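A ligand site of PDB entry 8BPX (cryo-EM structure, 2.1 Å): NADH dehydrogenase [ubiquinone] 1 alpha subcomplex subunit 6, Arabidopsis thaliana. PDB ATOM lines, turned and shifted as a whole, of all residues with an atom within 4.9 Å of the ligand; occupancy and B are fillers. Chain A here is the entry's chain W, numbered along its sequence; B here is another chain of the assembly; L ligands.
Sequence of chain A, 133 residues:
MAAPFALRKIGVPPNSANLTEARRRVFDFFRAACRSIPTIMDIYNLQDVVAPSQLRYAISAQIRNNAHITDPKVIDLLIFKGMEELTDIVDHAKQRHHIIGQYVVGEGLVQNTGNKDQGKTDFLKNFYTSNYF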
ATOM      1  N   ARG A  23      24.698  32.398  20.318  1.00  0.00           N
ATOM      2  CA  ARG A  23      25.125  32.129  18.942  1.00  0.00           C
ATOM      3  C   ARG A  23      26.629  31.896  18.876  1.00  0.00           C
ATOM      4  O   ARG A  23      27.096  31.038  18.117  1.00  0.00           O
ATOM      5  CB  ARG A  23      24.716  33.287  18.034  1.00  0.00           C
ATOM      6  CG  ARG A  23      25.087  33.099  16.571  1.00  0.00           C
ATOM      7  CD  ARG A  23      24.201  33.907  15.634  1.00  0.00           C
ATOM      8  NE  ARG A  23      23.657  35.110  16.271  1.00  0.00           N
ATOM      9  CZ  ARG A  23      22.365  35.358  16.408  1.00  0.00           C
ATOM     10  NH1 ARG A  23      21.449  34.514  15.976  1.00  0.00           N
ATOM     11  NH2 ARG A  23      21.987  36.499  16.991  1.00  0.00           N
ATOM     12  N   VAL A  26      27.217  28.493  19.922  1.00  0.00           N
ATOM     13  CA  VAL A  26      26.829  27.590  18.834  1.00  0.00           C
ATOM     14  C   VAL A  26      27.966  27.467  17.826  1.00  0.00           C
ATOM     15  O   VAL A  26      28.298  26.369  17.359  1.00  0.00           O
ATOM     16  CB  VAL A  26      25.538  28.087  18.148  1.00  0.00           C
ATOM     17  CG1 VAL A  26      25.262  27.243  16.908  1.00  0.00           C
ATOM     18  CG2 VAL A  26      24.361  28.012  19.088  1.00  0.00           C
ATOM     19  N   PHE A  27      28.552  28.604  17.434  1.00  0.00           N
ATOM     20  CA  PHE A  27      29.634  28.566  16.451  1.00  0.00           C
ATOM     21  C   PHE A  27      30.832  27.802  16.987  1.00  0.00           C
ATOM     22  O   PHE A  27      31.455  27.015  16.249  1.00  0.00           O
ATOM     23  CB  PHE A  27      30.018  29.989  16.038  1.00  0.00           C
ATOM     24  CG  PHE A  27      29.045  30.640  15.104  1.00  0.00           C
ATOM     25  CD1 PHE A  27      27.985  29.923  14.576  1.00  0.00           C
ATOM     26  CD2 PHE A  27      29.189  31.965  14.731  1.00  0.00           C
ATOM     27  CE1 PHE A  27      27.080  30.527  13.709  1.00  0.00           C
ATOM     28  CE2 PHE A  27      28.291  32.575  13.869  1.00  0.00           C
ATOM     29  CZ  PHE A  27      27.231  31.845  13.358  1.00  0.00           C
ATOM     30  N   PHE A  29      30.733  25.336  19.205  1.00  0.00           N
ATOM     31  CA  PHE A  29      30.400  23.917  19.186  1.00  0.00           C
ATOM     32  C   PHE A  29      30.490  23.357  17.773  1.00  0.00           C
ATOM     33  O   PHE A  29      30.945  22.222  17.583  1.00  0.00           O
ATOM     34  CB  PHE A  29      29.006  23.676  19.760  1.00  0.00           C
ATOM     35  CG  PHE A  29      28.462  22.325  19.407  1.00  0.00           C
ATOM     36  CD1 PHE A  29      28.909  21.191  20.072  1.00  0.00           C
ATOM     37  CD2 PHE A  29      27.526  22.177  18.394  1.00  0.00           C
ATOM     38  CE1 PHE A  29      28.426  19.953  19.750  1.00  0.00           C
ATOM     39  CE2 PHE A  29      27.046  20.927  18.059  1.00  0.00           C
ATOM     40  CZ  PHE A  29      27.488  19.816  18.750  1.00  0.00           C
ATOM     41  N   ALA A  33      32.833  20.298  16.571  1.00  0.00           N
ATOM     42  CA  ALA A  33      32.262  19.098  15.962  1.00  0.00           C
ATOM     43  C   ALA A  33      32.885  18.818  14.601  1.00  0.00           C
ATOM     44  O   ALA A  33      33.214  17.669  14.284  1.00  0.00           O
ATOM     45  CB  ALA A  33      30.746  19.240  15.834  1.00  0.00           C
ATOM     46  N   ILE A  40      36.652  10.689  13.605  1.00  0.00           N
ATOM     47  CA  ILE A  40      35.481   9.831  13.459  1.00  0.00           C
ATOM     48  C   ILE A  40      35.613   8.951  12.218  1.00  0.00           C
ATOM     49  O   ILE A  40      35.272   7.756  12.245  1.00  0.00           O
ATOM     50  CB  ILE A  40      34.203  10.683  13.423  1.00  0.00           C
ATOM     51  CG1 ILE A  40      33.911  11.224  14.822  1.00  0.00           C
ATOM     52  CG2 ILE A  40      33.028   9.888  12.885  1.00  0.00           C
ATOM     53  CD1 ILE A  40      33.000  12.417  14.847  1.00  0.00           C
ATOM     54  N   ILE A  59      25.823  17.781  10.479  1.00  0.00           N
ATOM     55  CA  ILE A  59      25.927  18.603  11.682  1.00  0.00           C
ATOM     56  C   ILE A  59      25.260  19.956  11.456  1.00  0.00           C
ATOM     57  O   ILE A  59      24.472  20.438  12.293  1.00  0.00           O
ATOM     58  CB  ILE A  59      27.391  18.770  12.103  1.00  0.00           C
ATOM     59  CG1 ILE A  59      28.026  17.420  12.429  1.00  0.00           C
ATOM     60  CG2 ILE A  59      27.507  19.678  13.312  1.00  0.00           C
ATOM     61  CD1 ILE A  59      29.512  17.511  12.673  1.00  0.00           C
ATOM     62  N   GLN A  62      21.514  19.686  11.425  1.00  0.00           N
ATOM     63  CA  GLN A  62      20.991  19.612  12.784  1.00  0.00           C
ATOM     64  C   GLN A  62      20.936  20.983  13.437  1.00  0.00           C
ATOM     65  O   GLN A  62      19.979  21.316  14.139  1.00  0.00           O
ATOM     66  CB  GLN A  62      21.846  18.650  13.624  1.00  0.00           C
ATOM     67  CG  GLN A  62      21.553  17.181  13.387  1.00  0.00           C
ATOM     68  CD  GLN A  62      20.195  16.725  13.906  1.00  0.00           C
ATOM     69  OE1 GLN A  62      19.473  17.508  14.529  1.00  0.00           O
ATOM     70  NE2 GLN A  62      19.819  15.483  13.622  1.00  0.00           N
ATOM     71  N   ILE A  63      21.968  21.800  13.202  1.00  0.00           N
ATOM     72  CA  ILE A  63      21.974  23.152  13.752  1.00  0.00           C
ATOM     73  C   ILE A  63      20.857  23.990  13.122  1.00  0.00           C
ATOM     74  O   ILE A  63      20.229  24.822  13.783  1.00  0.00           O
ATOM     75  CB  ILE A  63      23.356  23.800  13.557  1.00  0.00           C
ATOM     76  CG1 ILE A  63      24.400  23.075  14.399  1.00  0.00           C
ATOM     77  CG2 ILE A  63      23.315  25.289  13.929  1.00  0.00           C
ATOM     78  CD1 ILE A  63      25.794  23.632  14.261  1.00  0.00           C
ATOM     79  N   ARG A  64      20.594  23.779  11.837  1.00  0.00           N
ATOM     80  CA  ARG A  64      19.625  24.603  11.115  1.00  0.00           C
ATOM     81  C   ARG A  64      18.197  24.241  11.479  1.00  0.00           C
ATOM     82  O   ARG A  64      17.333  25.116  11.547  1.00  0.00           O
ATOM     83  CB  ARG A  64      19.839  24.482   9.612  1.00  0.00           C
ATOM     84  CG  ARG A  64      21.073  25.171   9.110  1.00  0.00           C
ATOM     85  CD  ARG A  64      20.777  26.068   7.932  1.00  0.00           C
ATOM     86  NE  ARG A  64      21.995  26.681   7.414  1.00  0.00           N
ATOM     87  CZ  ARG A  64      22.192  27.978   7.328  1.00  0.00           C
ATOM     88  NH1 ARG A  64      21.262  28.846   7.710  1.00  0.00           N
ATOM     89  NH2 ARG A  64      23.344  28.438   6.844  1.00  0.00           N
ATOM     90  N   ASN A  66      17.021  23.637  14.202  1.00  0.00           N
ATOM     91  CA  ASN A  66      16.689  24.321  15.449  1.00  0.00           C
ATOM     92  C   ASN A  66      16.900  25.832  15.359  1.00  0.00           C
ATOM     93  O   ASN A  66      17.038  26.498  16.380  1.00  0.00           O
ATOM     94  CB  ASN A  66      17.521  23.755  16.607  1.00  0.00           C
ATOM     95  CG  ASN A  66      17.092  22.373  17.014  1.00  0.00           C
ATOM     96  OD1 ASN A  66      17.894  21.438  17.016  1.00  0.00           O
ATOM     97  ND2 ASN A  66      15.825  22.226  17.362  1.00  0.00           N
ATOM     98  N   ALA A  67      16.921  26.379  14.139  1.00  0.00           N
ATOM     99  CA  ALA A  67      17.188  27.806  13.970  1.00  0.00           C
ATOM    100  C   ALA A  67      16.047  28.688  14.454  1.00  0.00           C
ATOM    101  O   ALA A  67      16.227  29.901  14.559  1.00  0.00           O
ATOM    102  CB  ALA A  67      17.491  28.110  12.504  1.00  0.00           C
ATOM    103  N   ILE A  69      14.702  28.518  17.450  1.00  0.00           N
ATOM    104  CA  ILE A  69      14.729  28.662  18.895  1.00  0.00           C
ATOM    105  C   ILE A  69      15.147  30.079  19.252  1.00  0.00           C
ATOM    106  O   ILE A  69      16.133  30.611  18.715  1.00  0.00           O
ATOM    107  CB  ILE A  69      15.673  27.624  19.517  1.00  0.00           C
ATOM    108  CG1 ILE A  69      15.120  26.208  19.341  1.00  0.00           C
ATOM    109  CG2 ILE A  69      15.898  27.937  20.992  1.00  0.00           C
ATOM    110  CD1 ILE A  69      13.630  26.098  19.540  1.00  0.00           C
ATOM    111  N   ILE A  75      19.006  26.948  23.890  1.00  0.00           N
ATOM    112  CA  ILE A  75      20.182  26.834  23.042  1.00  0.00           C
ATOM    113  C   ILE A  75      21.375  26.301  23.825  1.00  0.00           C
ATOM    114  O   ILE A  75      22.117  25.435  23.352  1.00  0.00           O
ATOM    115  CB  ILE A  75      20.505  28.191  22.391  1.00  0.00           C
ATOM    116  CG1 ILE A  75      19.369  28.599  21.442  1.00  0.00           C
ATOM    117  CG2 ILE A  75      21.831  28.147  21.672  1.00  0.00           C
ATOM    118  CD1 ILE A  75      19.559  29.967  20.834  1.00  0.00           C
ATOM    119  N   LEU A  78      20.855  22.613  24.362  1.00  0.00           N
ATOM    120  CA  LEU A  78      21.094  21.881  23.123  1.00  0.00           C
ATOM    121  C   LEU A  78      22.582  21.758  22.839  1.00  0.00           C
ATOM    122  O   LEU A  78      23.048  20.702  22.400  1.00  0.00           O
ATOM    123  CB  LEU A  78      20.356  22.559  21.965  1.00  0.00           C
ATOM    124  CG  LEU A  78      18.834  22.433  21.950  1.00  0.00           C
ATOM    125  CD1 LEU A  78      18.237  23.260  20.829  1.00  0.00           C
ATOM    126  CD2 LEU A  78      18.399  20.995  21.845  1.00  0.00           C
ATOM    127  N   ILE A  79      23.336  22.827  23.096  1.00  0.00           N
ATOM    128  CA  ILE A  79      24.787  22.778  22.894  1.00  0.00           C
ATOM    129  C   ILE A  79      25.432  21.793  23.859  1.00  0.00           C
ATOM    130  O   ILE A  79      26.342  21.037  23.478  1.00  0.00           O
ATOM    131  CB  ILE A  79      25.399  24.189  23.047  1.00  0.00           C
ATOM    132  CG1 ILE A  79      24.957  25.100  21.906  1.00  0.00           C
ATOM    133  CG2 ILE A  79      26.907  24.103  23.087  1.00  0.00           C
ATOM    134  CD1 ILE A  79      25.204  26.572  22.193  1.00  0.00           C
ATOM    135  N   GLY A  82      24.685  18.343  22.629  1.00  0.00           N
ATOM    136  CA  GLY A  82      25.492  18.072  21.448  1.00  0.00           C
ATOM    137  C   GLY A  82      26.936  17.751  21.798  1.00  0.00           C
ATOM    138  O   GLY A  82      27.534  16.846  21.217  1.00  0.00           O
ATOM    139  N   GLU A  85      27.010  14.206  23.198  1.00  0.00           N
ATOM    140  CA  GLU A  85      26.846  13.213  22.136  1.00  0.00           C
ATOM    141  C   GLU A  85      28.110  13.105  21.300  1.00  0.00           C
ATOM    142  O   GLU A  85      28.527  12.000  20.940  1.00  0.00           O
ATOM    143  CB  GLU A  85      25.644  13.572  21.270  1.00  0.00           C
ATOM    144  CG  GLU A  85      25.826  13.298  19.791  1.00  0.00           C
ATOM    145  CD  GLU A  85      24.504  13.122  19.068  1.00  0.00           C
ATOM    146  OE1 GLU A  85      23.509  13.749  19.483  1.00  0.00           O
ATOM    147  OE2 GLU A  85      24.456  12.336  18.104  1.00  0.00           O
ATOM    148  N   LEU A  86      28.750  14.236  20.993  1.00  0.00           N
ATOM    149  CA  LEU A  86      30.025  14.215  20.283  1.00  0.00           C
ATOM    150  C   LEU A  86      31.090  13.467  21.071  1.00  0.00           C
ATOM    151  O   LEU A  86      31.855  12.669  20.515  1.00  0.00           O
ATOM    152  CB  LEU A  86      30.484  15.636  19.986  1.00  0.00           C
ATOM    153  CG  LEU A  86      31.836  15.816  19.303  1.00  0.00           C
ATOM    154  CD1 LEU A  86      31.889  15.077  17.982  1.00  0.00           C
ATOM    155  CD2 LEU A  86      32.159  17.286  19.123  1.00  0.00           C
ATOM    156  N   ILE A  89      30.425   9.801  20.912  1.00  0.00           N
ATOM    157  CA  ILE A  89      30.727   9.295  19.570  1.00  0.00           C
ATOM    158  C   ILE A  89      32.226   9.107  19.404  1.00  0.00           C
ATOM    159  O   ILE A  89      32.679   8.090  18.861  1.00  0.00           O
ATOM    160  CB  ILE A  89      30.153  10.256  18.515  1.00  0.00           C
ATOM    161  CG1 ILE A  89      28.702   9.898  18.190  1.00  0.00           C
ATOM    162  CG2 ILE A  89      31.003  10.258  17.247  1.00  0.00           C
ATOM    163  CD1 ILE A  89      27.977  10.951  17.411  1.00  0.00           C
ATOM    164  N   ILE A 100      25.935   6.150  12.779  1.00  0.00           N
ATOM    165  CA  ILE A 100      26.843   6.685  13.840  1.00  0.00           C
ATOM    166  C   ILE A 100      25.937   7.371  14.864  1.00  0.00           C
ATOM    167  O   ILE A 100      25.163   8.203  14.449  1.00  0.00           O
ATOM    168  CB  ILE A 100      27.859   7.724  13.329  1.00  0.00           C
ATOM    169  CG1 ILE A 100      28.782   7.164  12.246  1.00  0.00           C
ATOM    170  CG2 ILE A 100      28.663   8.267  14.486  1.00  0.00           C
ATOM    171  CD1 ILE A 100      29.467   8.255  11.461  1.00  0.00           C
ATOM    172  N   TYR A 103      22.584   9.176  13.753  1.00  0.00           N
ATOM    173  CA  TYR A 103      22.512   9.467  12.298  1.00  0.00           C
ATOM    174  C   TYR A 103      22.843   8.281  11.401  1.00  0.00           C
ATOM    175  O   TYR A 103      23.834   7.602  11.619  1.00  0.00           O
ATOM    176  CB  TYR A 103      23.357  10.668  11.954  1.00  0.00           C
ATOM    177  CG  TYR A 103      23.276  11.698  13.045  1.00  0.00           C
ATOM    178  CD1 TYR A 103      22.165  12.508  13.191  1.00  0.00           C
ATOM    179  CD2 TYR A 103      24.289  11.803  13.986  1.00  0.00           C
ATOM    180  CE1 TYR A 103      22.069  13.423  14.224  1.00  0.00           C
ATOM    181  CE2 TYR A 103      24.209  12.718  15.015  1.00  0.00           C
ATOM    182  CZ  TYR A 103      23.105  13.533  15.142  1.00  0.00           C
ATOM    183  OH  TYR A 103      23.034  14.429  16.158  1.00  0.00           O
ATOM    184  N   ASP B  82      24.750  33.159   4.964  1.00  0.00           N
ATOM    185  CA  ASP B  82      24.618  33.647   6.332  1.00  0.00           C
ATOM    186  C   ASP B  82      25.894  33.319   7.123  1.00  0.00           C
ATOM    187  O   ASP B  82      26.828  32.693   6.620  1.00  0.00           O
ATOM    188  CB  ASP B  82      23.364  33.072   6.978  1.00  0.00           C
ATOM    189  CG  ASP B  82      23.325  31.554   6.976  1.00  0.00           C
ATOM    190  OD1 ASP B  82      24.400  30.912   7.049  1.00  0.00           O
ATOM    191  OD2 ASP B  82      22.212  30.996   6.899  1.00  0.00           O
ATOM    192  N   SER B  83      25.914  33.759   8.391  1.00  0.00           N
ATOM    193  CA  SER B  83      27.106  33.569   9.211  1.00  0.00           C
ATOM    194  C   SER B  83      27.421  32.092   9.416  1.00  0.00           C
ATOM    195  O   SER B  83      28.584  31.695   9.412  1.00  0.00           O
ATOM    196  CB  SER B  83      26.941  34.272  10.557  1.00  0.00           C
ATOM    197  OG  SER B  83      25.682  34.010  11.121  1.00  0.00           O
ATOM    198  N   LEU B  84      26.385  31.271   9.616  1.00  0.00           N
ATOM    199  CA  LEU B  84      26.610  29.836   9.723  1.00  0.00           C
ATOM    200  C   LEU B  84      27.254  29.282   8.462  1.00  0.00           C
ATOM    201  O   LEU B  84      28.199  28.486   8.533  1.00  0.00           O
ATOM    202  CB  LEU B  84      25.291  29.112  10.009  1.00  0.00           C
ATOM    203  CG  LEU B  84      25.422  27.592  10.179  1.00  0.00           C
ATOM    204  CD1 LEU B  84      26.495  27.276  11.207  1.00  0.00           C
ATOM    205  CD2 LEU B  84      24.097  26.969  10.578  1.00  0.00           C
HETATM  206  O1  LIG L   1      20.704  22.719  17.124  1.00  0.00           O
HETATM  207  C1  LIG L   1      28.755  13.060  14.085  1.00  0.00           C
HETATM  208  O2  LIG L   1      23.645  32.313  10.210  1.00  0.00           O
HETATM  209  C2  LIG L   1      28.135  14.280  14.731  1.00  0.00           C
HETATM  210  C3  LIG L   1      28.466  14.421  16.188  1.00  0.00           C
HETATM  211  C4  LIG L   1      27.905  15.661  16.828  1.00  0.00           C
HETATM  212  O3  LIG L   1      21.205  32.921  10.426  1.00  0.00           O
HETATM  213  C5  LIG L   1      26.413  15.822  16.681  1.00  0.00           C
HETATM  214  C6  LIG L   1      25.855  17.052  17.353  1.00  0.00           C
HETATM  215  C7  LIG L   1      24.390  17.295  17.095  1.00  0.00           C
HETATM  216  C8  LIG L   1      23.860  18.560  17.720  1.00  0.00           C
HETATM  217  C9  LIG L   1      22.388  18.785  17.499  1.00  0.00           C
HETATM  218  C10 LIG L   1      21.864  20.103  18.042  1.00  0.00           C
HETATM  219  C11 LIG L   1      22.571  21.293  17.489  1.00  0.00           C
HETATM  220  C12 LIG L   1      21.794  22.568  17.608  1.00  0.00           C
HETATM  221  C13 LIG L   1      22.781  30.941  12.580  1.00  0.00           C
HETATM  222  C14 LIG L   1      21.425  30.249  12.718  1.00  0.00           C
HETATM  223  C15 LIG L   1      20.919  29.857  11.326  1.00  0.00           C
HETATM  224  C16 LIG L   1      21.597  28.966  13.527  1.00  0.00           C
HETATM  225  C17 LIG L   1      20.400  31.177  13.399  1.00  0.00           C
HETATM  226  C18 LIG L   1      20.442  31.132  14.931  1.00  0.00           C
HETATM  227  C19 LIG L   1      19.285  30.450  16.980  1.00  0.00           C
HETATM  228  C20 LIG L   1      19.018  29.003  17.320  1.00  0.00           C
HETATM  229  C21 LIG L   1      20.260  28.132  17.250  1.00  0.00           C
HETATM  230  C22 LIG L   1      21.172  25.850  17.364  1.00  0.00           C
HETATM  231  C23 LIG L   1      21.363  25.102  18.663  1.00  0.00           C
HETATM  232  N1  LIG L   1      19.355  30.675  15.539  1.00  0.00           N
HETATM  233  N2  LIG L   1      20.091  26.822  17.453  1.00  0.00           N
HETATM  234  O4  LIG L   1      22.583  32.385  12.463  1.00  0.00           O
HETATM  235  O5  LIG L   1      19.099  30.844  12.950  1.00  0.00           O
HETATM  236  O6  LIG L   1      21.437  31.507  15.531  1.00  0.00           O
HETATM  237  O7  LIG L   1      21.364  28.624  16.999  1.00  0.00           O
HETATM  238  P1  LIG L   1      22.600  33.076  11.005  1.00  0.00           P
HETATM  239  S1  LIG L   1      22.630  23.805  18.555  1.00  0.00           S
HETATM  240  O8  LIG L   1      22.971  34.517  11.242  1.00  0.00           O
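The side-chain carboxylate (OD2) of Asp 82 of chain B is in salt-bridge range of the guanidinium group (NH1) of Arg 64, 2.5 Å away.
The backbone NH (N) of Leu 84 of chain B sits close to the side-chain carboxylate (OD1) of Asp 82 of chain B (3.3 Å).
OE2 of Glu 85 lies close to OH of Tyr 103 (3.2 Å).
An oxygen (O1) of the ligand sits close to the backbone carbonyl oxygen (O) of Gln 62, 3.4 Å away.
Val 26 touches the ligand.
CZ of Phe 29 touches C6 of the ligand, at 3.5 Å.
CG1 of Ile 59 touches C2 of the ligand, 3.9 Å away.
CA of Ile 63 touches O1 of the ligand (3.6 Å).
NH1 of Arg 64 touches C15 of the ligand (3.8 Å).
Ile 69 touches the ligand.
Ile 75 touches the ligand.
Leu 86 touches the ligand.
Ile 89 touches the ligand (CD1 to C3, 3.7 Å).
Tyr 103 touches the ligand.
Asp 82 of chain B touches the ligand.
Of the 25 residues printed, 17 come within 4 Å of the ligand.
The nearest printed residue that does not touch the ligand is Glu 85 (4.05 Å).
N of Ser 83 of chain B sits at hydrogen-bond distance from O2 of the ligand, 3.2 Å away.
The backbone carbonyl oxygen of Asn 66 lies within hydrogen-bond range of a nitrogen (N2) of the ligand (3.3 Å).
O of Ala 67 sits at hydrogen-bond distance from N1 of the ligand, at 3.4 Å.
N of Leu 84 of chain B lies within hydrogen-bond range of O2 of the ligand (3.0 Å).
The guanidinium group (NH1) of Arg 23 lies within hydrogen-bond range of an oxygen (O6) of the ligand (3.0 Å).
The side-chain hydroxyl (OG) of Ser 83 of chain B sits at hydrogen-bond distance from an oxygen (O8) of the ligand.
OD1 of Asn 66 lies close to O1 of the ligand, at 3.1 Å.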
